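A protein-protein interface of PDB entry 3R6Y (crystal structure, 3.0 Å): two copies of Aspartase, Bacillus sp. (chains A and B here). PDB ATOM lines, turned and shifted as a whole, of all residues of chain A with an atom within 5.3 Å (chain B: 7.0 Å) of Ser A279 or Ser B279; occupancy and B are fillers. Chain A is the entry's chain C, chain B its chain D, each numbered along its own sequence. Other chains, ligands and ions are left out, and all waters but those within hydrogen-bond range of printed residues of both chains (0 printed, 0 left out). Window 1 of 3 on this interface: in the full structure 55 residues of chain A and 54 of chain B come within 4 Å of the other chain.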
ATOM      1  N   THR A 275     -37.595 -14.873 -28.165  1.00  0.00           N
ATOM      2  CA  THR A 275     -36.213 -14.411 -28.194  1.00  0.00           C
ATOM      3  C   THR A 275     -35.610 -14.554 -26.800  1.00  0.00           C
ATOM      4  O   THR A 275     -34.394 -14.743 -26.646  1.00  0.00           O
ATOM      5  CB  THR A 275     -36.095 -12.960 -28.716  1.00  0.00           C
ATOM      6  OG1 THR A 275     -37.174 -12.171 -28.208  1.00  0.00           O
ATOM      7  CG2 THR A 275     -36.157 -12.941 -30.235  1.00  0.00           C
ATOM      8  N   GLU A 276     -36.480 -14.493 -25.794  1.00  0.00           N
ATOM      9  CA  GLU A 276     -36.093 -14.658 -24.397  1.00  0.00           C
ATOM     10  C   GLU A 276     -35.506 -16.047 -24.149  1.00  0.00           C
ATOM     11  O   GLU A 276     -34.472 -16.197 -23.491  1.00  0.00           O
ATOM     12  CB  GLU A 276     -37.325 -14.436 -23.519  1.00  0.00           C
ATOM     13  CG  GLU A 276     -37.070 -14.515 -22.030  1.00  0.00           C
ATOM     14  CD  GLU A 276     -38.268 -14.082 -21.219  1.00  0.00           C
ATOM     15  OE1 GLU A 276     -38.099 -13.832 -20.008  1.00  0.00           O
ATOM     16  OE2 GLU A 276     -39.374 -13.987 -21.788  1.00  0.00           O
ATOM     17  N   VAL A 277     -36.183 -17.052 -24.689  1.00  0.00           N
ATOM     18  CA  VAL A 277     -35.734 -18.436 -24.613  1.00  0.00           C
ATOM     19  C   VAL A 277     -34.384 -18.619 -25.307  1.00  0.00           C
ATOM     20  O   VAL A 277     -33.452 -19.158 -24.715  1.00  0.00           O
ATOM     21  CB  VAL A 277     -36.747 -19.387 -25.282  1.00  0.00           C
ATOM     22  CG1 VAL A 277     -36.372 -20.836 -25.026  1.00  0.00           C
ATOM     23  CG2 VAL A 277     -38.149 -19.109 -24.779  1.00  0.00           C
ATOM     24  N   SER A 278     -34.286 -18.180 -26.563  1.00  0.00           N
ATOM     25  CA  SER A 278     -33.046 -18.317 -27.341  1.00  0.00           C
ATOM     26  C   SER A 278     -31.848 -17.714 -26.603  1.00  0.00           C
ATOM     27  O   SER A 278     -30.733 -18.242 -26.664  1.00  0.00           O
ATOM     28  CB  SER A 278     -33.188 -17.656 -28.711  1.00  0.00           C
ATOM     29  OG  SER A 278     -32.064 -17.933 -29.530  1.00  0.00           O
ATOM     30  N   SER A 279     -32.098 -16.610 -25.903  1.00  0.00           N
ATOM     31  CA  SER A 279     -31.082 -15.968 -25.073  1.00  0.00           C
ATOM     32  C   SER A 279     -30.612 -16.843 -23.907  1.00  0.00           C
ATOM     33  O   SER A 279     -29.409 -16.921 -23.627  1.00  0.00           O
ATOM     34  CB  SER A 279     -31.619 -14.645 -24.545  1.00  0.00           C
ATOM     35  OG  SER A 279     -31.807 -13.745 -25.615  1.00  0.00           O
ATOM     36  N   ALA A 280     -31.554 -17.489 -23.222  1.00  0.00           N
ATOM     37  CA  ALA A 280     -31.201 -18.417 -22.143  1.00  0.00           C
ATOM     38  C   ALA A 280     -30.453 -19.629 -22.703  1.00  0.00           C
ATOM     39  O   ALA A 280     -29.537 -20.143 -22.056  1.00  0.00           O
ATOM     40  CB  ALA A 280     -32.434 -18.854 -21.375  1.00  0.00           C
ATOM     41  N   LEU A 281     -30.834 -20.066 -23.910  1.00  0.00           N
ATOM     42  CA  LEU A 281     -30.151 -21.166 -24.595  1.00  0.00           C
ATOM     43  C   LEU A 281     -28.757 -20.746 -25.048  1.00  0.00           C
ATOM     44  O   LEU A 281     -27.776 -21.422 -24.743  1.00  0.00           O
ATOM     45  CB  LEU A 281     -30.951 -21.666 -25.803  1.00  0.00           C
ATOM     46  CG  LEU A 281     -32.327 -22.306 -25.574  1.00  0.00           C
ATOM     47  CD1 LEU A 281     -32.769 -23.082 -26.809  1.00  0.00           C
ATOM     48  CD2 LEU A 281     -32.333 -23.218 -24.369  1.00  0.00           C
ATOM     49  N   LYS A 282     -28.661 -19.638 -25.778  1.00  0.00           N
ATOM     50  CA  LYS A 282     -27.360 -19.135 -26.210  1.00  0.00           C
ATOM     51  C   LYS A 282     -26.418 -19.115 -25.014  1.00  0.00           C
ATOM     52  O   LYS A 282     -25.351 -19.723 -25.050  1.00  0.00           O
ATOM     53  CB  LYS A 282     -27.486 -17.722 -26.783  1.00  0.00           C
ATOM     54  CG  LYS A 282     -26.216 -17.179 -27.471  1.00  0.00           C
ATOM     55  CD  LYS A 282     -25.963 -15.667 -27.228  1.00  0.00           C
ATOM     56  CE  LYS A 282     -27.260 -14.851 -27.091  1.00  0.00           C
ATOM     57  NZ  LYS A 282     -27.090 -13.384 -27.254  1.00  0.00           N
ATOM     58  N   VAL A 283     -26.833 -18.435 -23.947  1.00  0.00           N
ATOM     59  CA  VAL A 283     -25.966 -18.221 -22.783  1.00  0.00           C
ATOM     60  C   VAL A 283     -25.519 -19.554 -22.168  1.00  0.00           C
ATOM     61  O   VAL A 283     -24.372 -19.686 -21.736  1.00  0.00           O
ATOM     62  CB  VAL A 283     -26.637 -17.301 -21.721  1.00  0.00           C
ATOM     63  CG1 VAL A 283     -25.862 -17.306 -20.403  1.00  0.00           C
ATOM     64  CG2 VAL A 283     -26.722 -15.889 -22.240  1.00  0.00           C
ATOM     65  N   CYS A 284     -26.406 -20.545 -22.148  1.00  0.00           N
ATOM     66  CA  CYS A 284     -26.020 -21.875 -21.691  1.00  0.00           C
ATOM     67  C   CYS A 284     -24.896 -22.414 -22.551  1.00  0.00           C
ATOM     68  O   CYS A 284     -23.904 -22.917 -22.026  1.00  0.00           O
ATOM     69  CB  CYS A 284     -27.208 -22.841 -21.690  1.00  0.00           C
ATOM     70  SG  CYS A 284     -26.800 -24.516 -21.150  1.00  0.00           S
ATOM     71  N   ASP A 344     -29.800 -18.395 -32.919  1.00  0.00           N
ATOM     72  CA  ASP A 344     -30.227 -17.192 -32.201  1.00  0.00           C
ATOM     73  C   ASP A 344     -30.180 -15.899 -33.046  1.00  0.00           C
ATOM     74  O   ASP A 344     -31.033 -15.011 -32.875  1.00  0.00           O
ATOM     75  CB  ASP A 344     -29.379 -17.012 -30.944  1.00  0.00           C
ATOM     76  CG  ASP A 344     -29.810 -15.832 -30.126  1.00  0.00           C
ATOM     77  OD1 ASP A 344     -28.944 -15.039 -29.725  1.00  0.00           O
ATOM     78  OD2 ASP A 344     -31.026 -15.693 -29.905  1.00  0.00           O
ATOM     79  N   ARG B 214     -37.391  -8.310 -17.645  1.00  0.00           N
ATOM     80  CA  ARG B 214     -36.229  -9.136 -18.011  1.00  0.00           C
ATOM     81  C   ARG B 214     -34.907  -8.477 -17.616  1.00  0.00           C
ATOM     82  O   ARG B 214     -34.033  -9.118 -17.037  1.00  0.00           O
ATOM     83  CB  ARG B 214     -36.211  -9.418 -19.522  1.00  0.00           C
ATOM     84  CG  ARG B 214     -37.152 -10.516 -20.003  1.00  0.00           C
ATOM     85  CD  ARG B 214     -37.145 -10.627 -21.535  1.00  0.00           C
ATOM     86  NE  ARG B 214     -37.808  -9.486 -22.186  1.00  0.00           N
ATOM     87  CZ  ARG B 214     -39.041  -9.489 -22.711  1.00  0.00           C
ATOM     88  NH1 ARG B 214     -39.801 -10.589 -22.706  1.00  0.00           N
ATOM     89  NH2 ARG B 214     -39.524  -8.375 -23.260  1.00  0.00           N
ATOM     90  N   THR B 218     -31.556  -9.510 -14.476  1.00  0.00           N
ATOM     91  CA  THR B 218     -30.160  -9.711 -14.796  1.00  0.00           C
ATOM     92  C   THR B 218     -29.277  -9.193 -13.658  1.00  0.00           C
ATOM     93  O   THR B 218     -28.144  -9.649 -13.505  1.00  0.00           O
ATOM     94  CB  THR B 218     -29.771  -9.038 -16.146  1.00  0.00           C
ATOM     95  OG1 THR B 218     -29.740  -7.616 -16.000  1.00  0.00           O
ATOM     96  CG2 THR B 218     -30.757  -9.408 -17.250  1.00  0.00           C
ATOM     97  N   TYR B 274     -22.660 -11.467 -17.420  1.00  0.00           N
ATOM     98  CA  TYR B 274     -22.535 -10.437 -18.447  1.00  0.00           C
ATOM     99  C   TYR B 274     -23.343 -10.831 -19.684  1.00  0.00           C
ATOM    100  O   TYR B 274     -24.194 -10.076 -20.163  1.00  0.00           O
ATOM    101  CB  TYR B 274     -21.074 -10.224 -18.825  1.00  0.00           C
ATOM    102  CG  TYR B 274     -20.138  -9.983 -17.658  1.00  0.00           C
ATOM    103  CD1 TYR B 274     -19.083 -10.841 -17.418  1.00  0.00           C
ATOM    104  CD2 TYR B 274     -20.300  -8.894 -16.806  1.00  0.00           C
ATOM    105  CE1 TYR B 274     -18.214 -10.634 -16.362  1.00  0.00           C
ATOM    106  CE2 TYR B 274     -19.429  -8.679 -15.744  1.00  0.00           C
ATOM    107  CZ  TYR B 274     -18.391  -9.554 -15.536  1.00  0.00           C
ATOM    108  OH  TYR B 274     -17.505  -9.380 -14.514  1.00  0.00           O
ATOM    109  N   THR B 275     -23.089 -12.026 -20.190  1.00  0.00           N
ATOM    110  CA  THR B 275     -23.840 -12.521 -21.317  1.00  0.00           C
ATOM    111  C   THR B 275     -25.335 -12.494 -21.002  1.00  0.00           C
ATOM    112  O   THR B 275     -26.149 -12.266 -21.890  1.00  0.00           O
ATOM    113  CB  THR B 275     -23.394 -13.939 -21.678  1.00  0.00           C
ATOM    114  OG1 THR B 275     -23.659 -14.819 -20.578  1.00  0.00           O
ATOM    115  CG2 THR B 275     -21.898 -13.968 -21.993  1.00  0.00           C
ATOM    116  N   GLU B 276     -25.683 -12.714 -19.730  1.00  0.00           N
ATOM    117  CA  GLU B 276     -27.088 -12.638 -19.247  1.00  0.00           C
ATOM    118  C   GLU B 276     -27.686 -11.233 -19.412  1.00  0.00           C
ATOM    119  O   GLU B 276     -28.766 -11.069 -19.973  1.00  0.00           O
ATOM    120  CB  GLU B 276     -27.178 -13.085 -17.778  1.00  0.00           C
ATOM    121  CG  GLU B 276     -28.581 -13.005 -17.166  1.00  0.00           C
ATOM    122  CD  GLU B 276     -28.716 -13.699 -15.791  1.00  0.00           C
ATOM    123  OE1 GLU B 276     -29.756 -13.478 -15.120  1.00  0.00           O
ATOM    124  OE2 GLU B 276     -27.814 -14.471 -15.379  1.00  0.00           O
ATOM    125  N   VAL B 277     -26.965 -10.231 -18.919  1.00  0.00           N
ATOM    126  CA  VAL B 277     -27.346  -8.845 -19.106  1.00  0.00           C
ATOM    127  C   VAL B 277     -27.506  -8.555 -20.584  1.00  0.00           C
ATOM    128  O   VAL B 277     -28.559  -8.098 -21.020  1.00  0.00           O
ATOM    129  CB  VAL B 277     -26.281  -7.875 -18.544  1.00  0.00           C
ATOM    130  CG1 VAL B 277     -26.707  -6.422 -18.752  1.00  0.00           C
ATOM    131  CG2 VAL B 277     -26.031  -8.150 -17.075  1.00  0.00           C
ATOM    132  N   SER B 278     -26.458  -8.842 -21.349  1.00  0.00           N
ATOM    133  CA  SER B 278     -26.405  -8.515 -22.768  1.00  0.00           C
ATOM    134  C   SER B 278     -27.630  -8.983 -23.514  1.00  0.00           C
ATOM    135  O   SER B 278     -28.263  -8.215 -24.224  1.00  0.00           O
ATOM    136  CB  SER B 278     -25.176  -9.151 -23.408  1.00  0.00           C
ATOM    137  OG  SER B 278     -25.085  -8.807 -24.772  1.00  0.00           O
ATOM    138  N   SER B 279     -27.965 -10.251 -23.345  1.00  0.00           N
ATOM    139  CA  SER B 279     -29.052 -10.859 -24.108  1.00  0.00           C
ATOM    140  C   SER B 279     -30.420 -10.252 -23.788  1.00  0.00           C
ATOM    141  O   SER B 279     -31.311 -10.214 -24.647  1.00  0.00           O
ATOM    142  CB  SER B 279     -29.077 -12.356 -23.854  1.00  0.00           C
ATOM    143  OG  SER B 279     -27.795 -12.908 -24.083  1.00  0.00           O
ATOM    144  N   ALA B 280     -30.580  -9.796 -22.547  1.00  0.00           N
ATOM    145  CA  ALA B 280     -31.746  -9.040 -22.141  1.00  0.00           C
ATOM    146  C   ALA B 280     -31.795  -7.718 -22.906  1.00  0.00           C
ATOM    147  O   ALA B 280     -32.836  -7.335 -23.442  1.00  0.00           O
ATOM    148  CB  ALA B 280     -31.695  -8.788 -20.659  1.00  0.00           C
ATOM    149  N   LEU B 281     -30.658  -7.038 -22.969  1.00  0.00           N
ATOM    150  CA  LEU B 281     -30.542  -5.817 -23.757  1.00  0.00           C
ATOM    151  C   LEU B 281     -30.871  -6.047 -25.254  1.00  0.00           C
ATOM    152  O   LEU B 281     -31.590  -5.255 -25.869  1.00  0.00           O
ATOM    153  CB  LEU B 281     -29.146  -5.197 -23.584  1.00  0.00           C
ATOM    154  CG  LEU B 281     -28.711  -4.835 -22.150  1.00  0.00           C
ATOM    155  CD1 LEU B 281     -27.364  -4.113 -22.152  1.00  0.00           C
ATOM    156  CD2 LEU B 281     -29.740  -3.988 -21.417  1.00  0.00           C
ATOM    157  N   LYS B 282     -30.374  -7.133 -25.834  1.00  0.00           N
ATOM    158  CA  LYS B 282     -30.693  -7.458 -27.220  1.00  0.00           C
ATOM    159  C   LYS B 282     -32.191  -7.640 -27.427  1.00  0.00           C
ATOM    160  O   LYS B 282     -32.760  -7.108 -28.375  1.00  0.00           O
ATOM    161  CB  LYS B 282     -29.992  -8.740 -27.654  1.00  0.00           C
ATOM    162  CG  LYS B 282     -29.943  -8.937 -29.180  1.00  0.00           C
ATOM    163  CD  LYS B 282     -30.389 -10.347 -29.643  1.00  0.00           C
ATOM    164  CE  LYS B 282     -29.931 -11.482 -28.711  1.00  0.00           C
ATOM    165  NZ  LYS B 282     -29.703 -12.769 -29.419  1.00  0.00           N
ATOM    166  N   VAL B 283     -32.829  -8.410 -26.554  1.00  0.00           N
ATOM    167  CA  VAL B 283     -34.276  -8.621 -26.667  1.00  0.00           C
ATOM    168  C   VAL B 283     -35.021  -7.291 -26.587  1.00  0.00           C
ATOM    169  O   VAL B 283     -35.963  -7.064 -27.345  1.00  0.00           O
ATOM    170  CB  VAL B 283     -34.811  -9.605 -25.597  1.00  0.00           C
ATOM    171  CG1 VAL B 283     -36.256  -9.278 -25.207  1.00  0.00           C
ATOM    172  CG2 VAL B 283     -34.701 -11.046 -26.102  1.00  0.00           C
ATOM    173  N   CYS B 284     -34.587  -6.409 -25.688  1.00  0.00           N
ATOM    174  CA  CYS B 284     -35.224  -5.116 -25.561  1.00  0.00           C
ATOM    175  C   CYS B 284     -35.167  -4.392 -26.886  1.00  0.00           C
ATOM    176  O   CYS B 284     -36.205  -4.076 -27.464  1.00  0.00           O
ATOM    177  CB  CYS B 284     -34.589  -4.262 -24.468  1.00  0.00           C
ATOM    178  SG  CYS B 284     -35.532  -2.742 -24.095  1.00  0.00           S
ATOM    179  N   ASP B 344     -23.751  -7.440 -28.778  1.00  0.00           N
ATOM    180  CA  ASP B 344     -24.077  -8.723 -28.183  1.00  0.00           C
ATOM    181  C   ASP B 344     -23.218  -9.818 -28.753  1.00  0.00           C
ATOM    182  O   ASP B 344     -22.748 -10.661 -28.000  1.00  0.00           O
ATOM    183  CB  ASP B 344     -25.563  -9.063 -28.374  1.00  0.00           C
ATOM    184  CG  ASP B 344     -25.938 -10.430 -27.811  1.00  0.00           C
ATOM    185  OD1 ASP B 344     -26.643 -11.166 -28.524  1.00  0.00           O
ATOM    186  OD2 ASP B 344     -25.538 -10.774 -26.674  1.00  0.00           O
ATOM    187  N   ILE B 347     -19.729  -9.713 -27.203  1.00  0.00           N
ATOM    188  CA  ILE B 347     -19.826 -10.209 -25.833  1.00  0.00           C
ATOM    189  C   ILE B 347     -19.906 -11.737 -25.820  1.00  0.00           C
ATOM    190  O   ILE B 347     -19.262 -12.375 -24.983  1.00  0.00           O
ATOM    191  CB  ILE B 347     -21.042  -9.564 -25.104  1.00  0.00           C
ATOM    192  CG1 ILE B 347     -20.753  -8.083 -24.833  1.00  0.00           C
ATOM    193  CG2 ILE B 347     -21.357 -10.284 -23.804  1.00  0.00           C
ATOM    194  CD1 ILE B 347     -21.969  -7.213 -24.813  1.00  0.00           C
ATOM    195  N   THR B 348     -20.662 -12.312 -26.763  1.00  0.00           N
ATOM    196  CA  THR B 348     -20.777 -13.771 -26.886  1.00  0.00           C
ATOM    197  C   THR B 348     -19.451 -14.411 -27.242  1.00  0.00           C
ATOM    198  O   THR B 348     -19.017 -15.361 -26.598  1.00  0.00           O
ATOM    199  CB  THR B 348     -21.758 -14.204 -27.983  1.00  0.00           C
ATOM    200  OG1 THR B 348     -23.038 -13.603 -27.768  1.00  0.00           O
ATOM    201  CG2 THR B 348     -21.901 -15.730 -27.991  1.00  0.00           C
ATOM    202  N   LEU B 369     -20.738  -4.210 -23.279  1.00  0.00           N
ATOM    203  CA  LEU B 369     -21.838  -4.242 -22.305  1.00  0.00           C
ATOM    204  C   LEU B 369     -22.177  -2.847 -21.759  1.00  0.00           C
ATOM    205  O   LEU B 369     -23.347  -2.489 -21.657  1.00  0.00           O
ATOM    206  CB  LEU B 369     -21.510  -5.184 -21.137  1.00  0.00           C
ATOM    207  CG  LEU B 369     -22.619  -5.473 -20.105  1.00  0.00           C
ATOM    208  CD1 LEU B 369     -23.742  -6.312 -20.725  1.00  0.00           C
ATOM    209  CD2 LEU B 369     -22.065  -6.175 -18.863  1.00  0.00           C
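The side-chain carboxylate of Glu A276 is in salt-bridge range of the guanidinium group of Arg B214.
The side-chain amino group (NZ) of Lys A282 is in hydrogen-bond range of the side-chain hydroxyl (OG) of Ser B279 (3.3 Å).
The side-chain amino group (NZ) of Lys A282 is in salt-bridge range of the side-chain carboxylate (OD1) of Asp B344, 2.6 Å away.
The side-chain amino group (NZ) of Lys B282 lies within salt-bridge range of the side-chain carboxylate (OD1) of Asp A344 (2.4 Å).
The side-chain amino group of Lys A282 sits close to the side-chain amino group of Lys B282, at 3.4 Å.
O of Thr A275 lies within hydrogen-bond range of OG of Ser A279 (3.0 Å).
OG of Ser A278 lies within hydrogen-bond range of OD2 of Asp A344 (2.5 Å).
The side-chain amino group (NZ) of Lys A282 lies within salt-bridge range of the side-chain carboxylate (OD1) of Asp A344, 3.5 Å away.
The backbone carbonyl oxygen (O) of Thr B275 sits at hydrogen-bond distance from the side-chain hydroxyl (OG) of Ser B279 (2.8 Å).
The side-chain amino group (NZ) of Lys B282 is in salt-bridge range of the side-chain carboxylate (OD1) of Asp B344 (3.6 Å).
The backbone carbonyl oxygen of Asp B344 lies within hydrogen-bond range of the side-chain hydroxyl of Thr B348, at 3.0 Å.
Among the printed residues, pairs that only touch across the chains: Thr A275 with Val B283, Glu A276 with Val B283, Ser A279 with Ser B279, Ser A279 with Val B283, Lys A282 with Thr B348, Val A283 with Thr B275 and Val A283 with Ser B279.
Of the printed residues of chain B, Ser A279 touches Ser B279 (3.5 Å) and Val B283 (3.99 Å).
Ser B279 touches just these residues of chain A: Ser A279, Lys A282 and Val A283.
Of the printed residues of chain A, Thr B348 touches Lys A282 (3.6 Å).
Of the printed residues of chain A, Val B283 touches Thr A275, Glu A276 and Ser A279.
Printed residues of chain A within 4 Å of Thr B275: Val A283.
Val B277 touches none of the printed residues of chain A.
The nearest printed residue of chain B that does not touch Ser A279 is Lys B282 (4.3 Å).
Printed residues of chain A that touch a printed residue of chain B: Thr A275, Glu A276, Ser A279, Lys A282, Val A283 and Asp A344.
Hydrophobic or aromatic side chains of chain B within 4 Å of the printed part of chain A: Val B283.
Among the printed residues, Asp or Glu carboxylates within 4 Å of a Lys or Arg side-chain nitrogen of the other chain: Glu A276 with Arg B214 (3.5 Å), Lys A282 with Asp B344 (2.6 Å) and Asp A344 with Lys B282 (2.4 Å).
Glu A276 touches Val B283, but with the chains exchanged Val A283 does not touch Glu B276 (4.2 Å).
Ser A279 touches Val B283, and with the chains exchanged Val A283 touches Ser B279.
Lys A282 touches Ser B279, but with the chains exchanged Ser A279 does not touch Lys B282 (4.3 Å).
Lys A282 touches its own counterpart, Lys B282.
Of the 12 pairs that touch across the chains among the printed residues, 8 have their exchanged pair printed and touching as well.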
